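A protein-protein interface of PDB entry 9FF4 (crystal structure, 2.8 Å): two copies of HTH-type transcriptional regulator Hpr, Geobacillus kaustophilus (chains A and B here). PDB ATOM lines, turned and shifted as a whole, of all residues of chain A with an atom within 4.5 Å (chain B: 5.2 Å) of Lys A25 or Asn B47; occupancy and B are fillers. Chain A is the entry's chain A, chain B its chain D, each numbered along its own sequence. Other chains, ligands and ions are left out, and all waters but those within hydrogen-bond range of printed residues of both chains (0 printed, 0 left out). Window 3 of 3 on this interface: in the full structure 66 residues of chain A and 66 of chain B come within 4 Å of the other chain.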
ATOM      1  N   ALA A  21     -21.610   8.368  15.968  1.00  0.00           N
ATOM      2  CA  ALA A  21     -20.412   8.386  16.804  1.00  0.00           C
ATOM      3  C   ALA A  21     -19.997   9.821  17.114  1.00  0.00           C
ATOM      4  O   ALA A  21     -19.710  10.170  18.267  1.00  0.00           O
ATOM      5  CB  ALA A  21     -19.270   7.633  16.116  1.00  0.00           C
ATOM      6  N   GLN A  22     -19.994  10.673  16.091  1.00  0.00           N
ATOM      7  CA  GLN A  22     -19.687  12.082  16.288  1.00  0.00           C
ATOM      8  C   GLN A  22     -20.746  12.772  17.142  1.00  0.00           C
ATOM      9  O   GLN A  22     -20.418  13.611  17.998  1.00  0.00           O
ATOM     10  CB  GLN A  22     -19.576  12.783  14.938  1.00  0.00           C
ATOM     11  CG  GLN A  22     -19.087  14.182  15.078  1.00  0.00           C
ATOM     12  CD  GLN A  22     -17.587  14.197  15.201  1.00  0.00           C
ATOM     13  OE1 GLN A  22     -16.899  13.511  14.437  1.00  0.00           O
ATOM     14  NE2 GLN A  22     -17.063  14.955  16.173  1.00  0.00           N
ATOM     15  N   LEU A  23     -22.025  12.452  16.911  1.00  0.00           N
ATOM     16  CA  LEU A  23     -23.066  13.052  17.728  1.00  0.00           C
ATOM     17  C   LEU A  23     -22.937  12.610  19.173  1.00  0.00           C
ATOM     18  O   LEU A  23     -22.930  13.447  20.083  1.00  0.00           O
ATOM     19  CB  LEU A  23     -24.439  12.697  17.200  1.00  0.00           C
ATOM     20  CG  LEU A  23     -24.982  13.712  16.225  1.00  0.00           C
ATOM     21  CD1 LEU A  23     -26.214  13.125  15.662  1.00  0.00           C
ATOM     22  CD2 LEU A  23     -25.278  15.059  16.900  1.00  0.00           C
ATOM     23  N   SER A  24     -22.829  11.304  19.424  1.00  0.00           N
ATOM     24  CA  SER A  24     -22.901  10.903  20.820  1.00  0.00           C
ATOM     25  C   SER A  24     -21.670  11.382  21.570  1.00  0.00           C
ATOM     26  O   SER A  24     -21.740  11.642  22.776  1.00  0.00           O
ATOM     27  CB  SER A  24     -23.091   9.379  20.958  1.00  0.00           C
ATOM     28  OG  SER A  24     -22.161   8.614  20.219  1.00  0.00           O
ATOM     29  N   LYS A  25     -20.538  11.512  20.866  1.00  0.00           N
ATOM     30  CA  LYS A  25     -19.349  12.089  21.484  1.00  0.00           C
ATOM     31  C   LYS A  25     -19.603  13.541  21.854  1.00  0.00           C
ATOM     32  O   LYS A  25     -19.474  13.933  23.026  1.00  0.00           O
ATOM     33  CB  LYS A  25     -18.153  11.994  20.543  1.00  0.00           C
ATOM     34  CG  LYS A  25     -16.824  12.146  21.253  1.00  0.00           C
ATOM     35  CD  LYS A  25     -15.665  12.011  20.278  1.00  0.00           C
ATOM     36  CE  LYS A  25     -14.313  11.980  20.974  1.00  0.00           C
ATOM     37  NZ  LYS A  25     -13.329  12.161  19.917  1.00  0.00           N
ATOM     38  N   ALA A  26     -20.005  14.342  20.862  1.00  0.00           N
ATOM     39  CA  ALA A  26     -20.372  15.734  21.099  1.00  0.00           C
ATOM     40  C   ALA A  26     -21.320  15.861  22.276  1.00  0.00           C
ATOM     41  O   ALA A  26     -21.013  16.527  23.273  1.00  0.00           O
ATOM     42  CB  ALA A  26     -21.019  16.315  19.853  1.00  0.00           C
ATOM     43  N   LEU A  27     -22.476  15.220  22.182  1.00  0.00           N
ATOM     44  CA  LEU A  27     -23.427  15.297  23.273  1.00  0.00           C
ATOM     45  C   LEU A  27     -22.776  14.908  24.600  1.00  0.00           C
ATOM     46  O   LEU A  27     -22.735  15.717  25.530  1.00  0.00           O
ATOM     47  CB  LEU A  27     -24.624  14.424  22.956  1.00  0.00           C
ATOM     48  CG  LEU A  27     -25.843  14.840  23.741  1.00  0.00           C
ATOM     49  CD1 LEU A  27     -26.193  16.313  23.532  1.00  0.00           C
ATOM     50  CD2 LEU A  27     -26.894  13.928  23.211  1.00  0.00           C
ATOM     51  N   TRP A  28     -22.203  13.702  24.694  1.00  0.00           N
ATOM     52  CA  TRP A  28     -21.718  13.244  25.996  1.00  0.00           C
ATOM     53  C   TRP A  28     -20.683  14.199  26.584  1.00  0.00           C
ATOM     54  O   TRP A  28     -20.661  14.412  27.800  1.00  0.00           O
ATOM     55  CB  TRP A  28     -21.122  11.826  25.934  1.00  0.00           C
ATOM     56  CG  TRP A  28     -20.390  11.485  27.223  1.00  0.00           C
ATOM     57  CD1 TRP A  28     -19.062  11.201  27.366  1.00  0.00           C
ATOM     58  CD2 TRP A  28     -20.946  11.440  28.540  1.00  0.00           C
ATOM     59  NE1 TRP A  28     -18.754  10.972  28.686  1.00  0.00           N
ATOM     60  CE2 TRP A  28     -19.896  11.111  29.429  1.00  0.00           C
ATOM     61  CE3 TRP A  28     -22.229  11.651  29.060  1.00  0.00           C
ATOM     62  CZ2 TRP A  28     -20.094  10.967  30.805  1.00  0.00           C
ATOM     63  CZ3 TRP A  28     -22.423  11.521  30.426  1.00  0.00           C
ATOM     64  CH2 TRP A  28     -21.360  11.175  31.284  1.00  0.00           C
ATOM     65  N   LYS A  29     -19.800  14.766  25.757  1.00  0.00           N
ATOM     66  CA  LYS A  29     -18.727  15.583  26.336  1.00  0.00           C
ATOM     67  C   LYS A  29     -19.260  16.886  26.950  1.00  0.00           C
ATOM     68  O   LYS A  29     -18.822  17.286  28.037  1.00  0.00           O
ATOM     69  CB  LYS A  29     -17.627  15.873  25.302  1.00  0.00           C
ATOM     70  CG  LYS A  29     -16.596  14.742  25.140  1.00  0.00           C
ATOM     71  CD  LYS A  29     -15.994  14.423  26.506  1.00  0.00           C
ATOM     72  CE  LYS A  29     -14.770  13.530  26.431  1.00  0.00           C
ATOM     73  NZ  LYS A  29     -14.128  13.385  27.778  1.00  0.00           N
ATOM     74  N   TRP B  28     -22.952   6.878  24.432  1.00  0.00           N
ATOM     75  CA  TRP B  28     -21.533   7.070  24.153  1.00  0.00           C
ATOM     76  C   TRP B  28     -20.717   5.840  24.565  1.00  0.00           C
ATOM     77  O   TRP B  28     -19.678   5.533  23.957  1.00  0.00           O
ATOM     78  CB  TRP B  28     -20.990   8.332  24.847  1.00  0.00           C
ATOM     79  CG  TRP B  28     -19.482   8.388  24.758  1.00  0.00           C
ATOM     80  CD1 TRP B  28     -18.607   8.303  25.787  1.00  0.00           C
ATOM     81  CD2 TRP B  28     -18.688   8.460  23.559  1.00  0.00           C
ATOM     82  NE1 TRP B  28     -17.316   8.328  25.313  1.00  0.00           N
ATOM     83  CE2 TRP B  28     -17.343   8.415  23.948  1.00  0.00           C
ATOM     84  CE3 TRP B  28     -18.992   8.565  22.198  1.00  0.00           C
ATOM     85  CZ2 TRP B  28     -16.301   8.494  23.034  1.00  0.00           C
ATOM     86  CZ3 TRP B  28     -17.959   8.638  21.293  1.00  0.00           C
ATOM     87  CH2 TRP B  28     -16.630   8.609  21.711  1.00  0.00           C
ATOM     88  N   TRP B  35     -15.875   1.225  19.091  1.00  0.00           N
ATOM     89  CA  TRP B  35     -14.855   1.973  18.360  1.00  0.00           C
ATOM     90  C   TRP B  35     -13.448   1.537  18.772  1.00  0.00           C
ATOM     91  O   TRP B  35     -12.552   1.428  17.927  1.00  0.00           O
ATOM     92  CB  TRP B  35     -15.066   3.463  18.617  1.00  0.00           C
ATOM     93  CG  TRP B  35     -14.304   4.442  17.764  1.00  0.00           C
ATOM     94  CD1 TRP B  35     -13.222   4.195  16.976  1.00  0.00           C
ATOM     95  CD2 TRP B  35     -14.551   5.845  17.681  1.00  0.00           C
ATOM     96  NE1 TRP B  35     -12.800   5.353  16.377  1.00  0.00           N
ATOM     97  CE2 TRP B  35     -13.600   6.385  16.797  1.00  0.00           C
ATOM     98  CE3 TRP B  35     -15.498   6.698  18.260  1.00  0.00           C
ATOM     99  CZ2 TRP B  35     -13.558   7.757  16.484  1.00  0.00           C
ATOM    100  CZ3 TRP B  35     -15.460   8.046  17.952  1.00  0.00           C
ATOM    101  CH2 TRP B  35     -14.495   8.567  17.074  1.00  0.00           C
ATOM    102  N   ASN B  45      -5.792   4.696  19.359  1.00  0.00           N
ATOM    103  CA  ASN B  45      -6.891   4.990  20.271  1.00  0.00           C
ATOM    104  C   ASN B  45      -7.929   5.869  19.588  1.00  0.00           C
ATOM    105  O   ASN B  45      -7.715   6.387  18.487  1.00  0.00           O
ATOM    106  CB  ASN B  45      -6.390   5.647  21.553  1.00  0.00           C
ATOM    107  CG  ASN B  45      -5.675   6.967  21.291  1.00  0.00           C
ATOM    108  OD1 ASN B  45      -6.138   7.827  20.542  1.00  0.00           O
ATOM    109  ND2 ASN B  45      -4.500   7.100  21.874  1.00  0.00           N
ATOM    110  N   ILE B  46      -9.072   6.016  20.255  1.00  0.00           N
ATOM    111  CA  ILE B  46     -10.196   6.723  19.642  1.00  0.00           C
ATOM    112  C   ILE B  46      -9.774   8.126  19.212  1.00  0.00           C
ATOM    113  O   ILE B  46      -9.979   8.538  18.063  1.00  0.00           O
ATOM    114  CB  ILE B  46     -11.408   6.776  20.595  1.00  0.00           C
ATOM    115  CG1 ILE B  46     -11.923   5.376  20.912  1.00  0.00           C
ATOM    116  CG2 ILE B  46     -12.545   7.524  19.950  1.00  0.00           C
ATOM    117  CD1 ILE B  46     -13.140   5.405  21.805  1.00  0.00           C
ATOM    118  N   ASN B  47      -9.168   8.880  20.116  1.00  0.00           N
ATOM    119  CA  ASN B  47      -8.851  10.251  19.747  1.00  0.00           C
ATOM    120  C   ASN B  47      -7.775  10.325  18.687  1.00  0.00           C
ATOM    121  O   ASN B  47      -7.711  11.307  17.952  1.00  0.00           O
ATOM    122  CB  ASN B  47      -8.444  11.058  20.961  1.00  0.00           C
ATOM    123  CG  ASN B  47      -9.618  11.755  21.563  1.00  0.00           C
ATOM    124  OD1 ASN B  47     -10.545  12.145  20.860  1.00  0.00           O
ATOM    125  ND2 ASN B  47      -9.613  11.884  22.867  1.00  0.00           N
ATOM    126  N   GLU B  48      -6.891   9.332  18.617  1.00  0.00           N
ATOM    127  CA  GLU B  48      -5.931   9.305  17.518  1.00  0.00           C
ATOM    128  C   GLU B  48      -6.643   9.019  16.195  1.00  0.00           C
ATOM    129  O   GLU B  48      -6.322   9.613  15.153  1.00  0.00           O
ATOM    130  CB  GLU B  48      -4.861   8.247  17.788  1.00  0.00           C
ATOM    131  CG  GLU B  48      -3.884   8.547  18.927  1.00  0.00           C
ATOM    132  CD  GLU B  48      -2.954   7.343  19.231  1.00  0.00           C
ATOM    133  OE1 GLU B  48      -3.326   6.173  18.935  1.00  0.00           O
ATOM    134  OE2 GLU B  48      -1.839   7.577  19.751  1.00  0.00           O
ATOM    135  N   HIS B  49      -7.620   8.108  16.223  1.00  0.00           N
ATOM    136  CA  HIS B  49      -8.329   7.744  15.007  1.00  0.00           C
ATOM    137  C   HIS B  49      -9.205   8.886  14.545  1.00  0.00           C
ATOM    138  O   HIS B  49      -9.356   9.123  13.340  1.00  0.00           O
ATOM    139  CB  HIS B  49      -9.172   6.484  15.233  1.00  0.00           C
ATOM    140  CG  HIS B  49      -9.774   5.953  13.972  1.00  0.00           C
ATOM    141  ND1 HIS B  49     -11.130   5.964  13.733  1.00  0.00           N
ATOM    142  CD2 HIS B  49      -9.201   5.434  12.860  1.00  0.00           C
ATOM    143  CE1 HIS B  49     -11.368   5.451  12.538  1.00  0.00           C
ATOM    144  NE2 HIS B  49     -10.213   5.131  11.983  1.00  0.00           N
ATOM    145  N   HIS B  50      -9.811   9.587  15.501  1.00  0.00           N
ATOM    146  CA  HIS B  50     -10.546  10.800  15.175  1.00  0.00           C
ATOM    147  C   HIS B  50      -9.649  11.810  14.460  1.00  0.00           C
ATOM    148  O   HIS B  50      -9.992  12.298  13.372  1.00  0.00           O
ATOM    149  CB  HIS B  50     -11.125  11.390  16.452  1.00  0.00           C
ATOM    150  CG  HIS B  50     -12.480  11.970  16.263  1.00  0.00           C
ATOM    151  ND1 HIS B  50     -13.333  12.226  17.312  1.00  0.00           N
ATOM    152  CD2 HIS B  50     -13.136  12.341  15.140  1.00  0.00           C
ATOM    153  CE1 HIS B  50     -14.460  12.727  16.845  1.00  0.00           C
ATOM    154  NE2 HIS B  50     -14.365  12.814  15.529  1.00  0.00           N
ATOM    155  N   ILE B  51      -8.472  12.093  15.036  1.00  0.00           N
ATOM    156  CA  ILE B  51      -7.529  13.024  14.413  1.00  0.00           C
ATOM    157  C   ILE B  51      -7.238  12.627  12.965  1.00  0.00           C
ATOM    158  O   ILE B  51      -7.151  13.493  12.082  1.00  0.00           O
ATOM    159  CB  ILE B  51      -6.230  13.116  15.225  1.00  0.00           C
ATOM    160  CG1 ILE B  51      -6.515  13.503  16.658  1.00  0.00           C
ATOM    161  CG2 ILE B  51      -5.388  14.188  14.652  1.00  0.00           C
ATOM    162  CD1 ILE B  51      -5.392  13.140  17.631  1.00  0.00           C
ATOM    163  N   GLY B  70     -12.994  17.283  16.618  1.00  0.00           N
ATOM    164  CA  GLY B  70     -12.925  16.007  17.295  1.00  0.00           C
ATOM    165  C   GLY B  70     -13.285  16.044  18.759  1.00  0.00           C
ATOM    166  O   GLY B  70     -12.829  15.170  19.506  1.00  0.00           O
ATOM    167  N   VAL B  71     -14.069  17.035  19.198  1.00  0.00           N
ATOM    168  CA  VAL B  71     -14.514  17.147  20.583  1.00  0.00           C
ATOM    169  C   VAL B  71     -13.403  16.795  21.552  1.00  0.00           C
ATOM    170  O   VAL B  71     -13.571  15.898  22.383  1.00  0.00           O
ATOM    171  CB  VAL B  71     -15.709  16.223  20.844  1.00  0.00           C
ATOM    172  CG1 VAL B  71     -16.494  16.702  22.052  1.00  0.00           C
ATOM    173  CG2 VAL B  71     -16.567  16.124  19.608  1.00  0.00           C
ATOM    174  N   MET B  72     -12.247  17.436  21.433  1.00  0.00           N
ATOM    175  CA  MET B  72     -11.197  17.172  22.402  1.00  0.00           C
ATOM    176  C   MET B  72     -10.441  18.450  22.713  1.00  0.00           C
ATOM    177  O   MET B  72     -10.396  19.387  21.918  1.00  0.00           O
ATOM    178  CB  MET B  72     -10.217  16.070  21.935  1.00  0.00           C
ATOM    179  CG  MET B  72      -9.443  16.410  20.695  1.00  0.00           C
ATOM    180  SD  MET B  72      -8.407  15.049  20.160  1.00  0.00           S
ATOM    181  CE  MET B  72      -9.289  14.421  18.733  1.00  0.00           C
ATOM    182  N   THR B  76      -4.797  17.561  24.225  1.00  0.00           N
ATOM    183  CA  THR B  76      -4.842  16.163  23.844  1.00  0.00           C
ATOM    184  C   THR B  76      -4.631  16.007  22.352  1.00  0.00           C
ATOM    185  O   THR B  76      -3.962  15.065  21.905  1.00  0.00           O
ATOM    186  CB  THR B  76      -6.164  15.530  24.261  1.00  0.00           C
ATOM    187  OG1 THR B  76      -7.154  15.727  23.231  1.00  0.00           O
ATOM    188  CG2 THR B  76      -6.628  16.096  25.604  1.00  0.00           C
ATOM    189  N   PHE B  80      -1.571  13.701  21.168  1.00  0.00           N
ATOM    190  CA  PHE B  80      -1.876  12.554  20.327  1.00  0.00           C
ATOM    191  C   PHE B  80      -1.493  12.820  18.874  1.00  0.00           C
ATOM    192  O   PHE B  80      -1.083  11.897  18.169  1.00  0.00           O
ATOM    193  CB  PHE B  80      -3.351  12.172  20.469  1.00  0.00           C
ATOM    194  CG  PHE B  80      -3.702  11.556  21.819  1.00  0.00           C
ATOM    195  CD1 PHE B  80      -2.804  11.573  22.875  1.00  0.00           C
ATOM    196  CD2 PHE B  80      -4.924  10.960  22.025  1.00  0.00           C
ATOM    197  CE1 PHE B  80      -3.126  11.017  24.100  1.00  0.00           C
ATOM    198  CE2 PHE B  80      -5.247  10.397  23.249  1.00  0.00           C
ATOM    199  CZ  PHE B  80      -4.342  10.430  24.284  1.00  0.00           C
ATOM    200  N   TYR B 156     -22.356  23.617  19.676  1.00  0.00           N
ATOM    201  CA  TYR B 156     -21.032  23.715  19.066  1.00  0.00           C
ATOM    202  C   TYR B 156     -20.943  24.724  17.922  1.00  0.00           C
ATOM    203  O   TYR B 156     -19.835  25.154  17.581  1.00  0.00           O
ATOM    204  CB  TYR B 156     -20.584  22.321  18.558  1.00  0.00           C
ATOM    205  CG  TYR B 156     -20.317  21.327  19.677  1.00  0.00           C
ATOM    206  CD1 TYR B 156     -21.330  20.515  20.189  1.00  0.00           C
ATOM    207  CD2 TYR B 156     -19.064  21.232  20.251  1.00  0.00           C
ATOM    208  CE1 TYR B 156     -21.082  19.615  21.230  1.00  0.00           C
ATOM    209  CE2 TYR B 156     -18.810  20.333  21.291  1.00  0.00           C
ATOM    210  CZ  TYR B 156     -19.819  19.522  21.768  1.00  0.00           C
ATOM    211  OH  TYR B 156     -19.578  18.627  22.789  1.00  0.00           O
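Of the 15 printed residues of chain B, 6 touch a printed residue of chain A. Printed residues of chain B that touch a printed residue of chain A: Trp B28, Asn B47, His B50, Gly B70, Val B71 and Tyr B156. Hydrophobic or aromatic side chains of chain B that line the printed part of chain A: Trp B28, His B50, Val B71 and Tyr B156. Among the printed residues, no Asp or Glu carboxylate lies within 4 Å of a Lys or Arg side-chain nitrogen of the other chain.
OG of Ser A24 sits at hydrogen-bond distance from O of Ala A21. The side-chain amide oxygen (OD1) of Asn B45 sits at hydrogen-bond distance from the backbone NH (N) of Asn B47 (3.2 Å). The side-chain amide oxygen of Asn B47 lies close to the side-chain sulfur of Met B72 (3.7 Å).
Trp B28 touches its own counterpart, Trp A28. 1 position is printed for both chains. Of the 11 pairs that touch across the chains among the printed residues, 1 has its exchanged pair printed and touching as well.
Lys A25 touches just these residues of chain B: Trp B28 (3.4 Å), Asn B47 (2.9 Å), His B50 (2.6 Å) and Gly B70 (3.1 Å). Of chain A, only Lys A25 comes within 4 Å of Asn B47. Of the printed residues of chain A, Val B71 touches Gln A22 and Lys A29. Of the printed residues of chain A, His B50 touches Gln A22 (2.8 Å) and Lys A25 (2.6 Å). Printed residues of chain B within 4 Å of Lys A29: Val B71 (3.5 Å). Printed residues of chain A within 4 Å of Tyr B156: Ala A26 (2.6 Å). Of the printed residues of chain B, Ala A21 touches Trp B28 (3.8 Å). Leu A23 touches none of the printed residues of chain B. The nearest printed residue of chain A that does not touch Gly B70 is Gln A22 (4.4 Å).
NE2 of His B50 sits at hydrogen-bond distance from OE1 of Gln A22 (2.8 Å). NZ of Lys A25 lies within hydrogen-bond range of OD1 of Asn B47, at 2.9 Å. NZ of Lys A25 is in hydrogen-bond range of ND1 of His B50 (2.6 Å). The backbone carbonyl oxygen of Gly B70 lies within hydrogen-bond range of the side-chain amino group of Lys A25 (3.1 Å). The backbone carbonyl oxygen of Ala A26 sits at hydrogen-bond distance from the side-chain hydroxyl of Tyr B156, at 2.6 Å.
Among the printed residues, merely in contact across the chains: Trp A28 with Trp B28, Lys A25 with Trp B28, Lys A29 with Val B71, Gln A22 with Val B71, Ser A24 with Trp B28 and Ala A21 with Trp B28.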
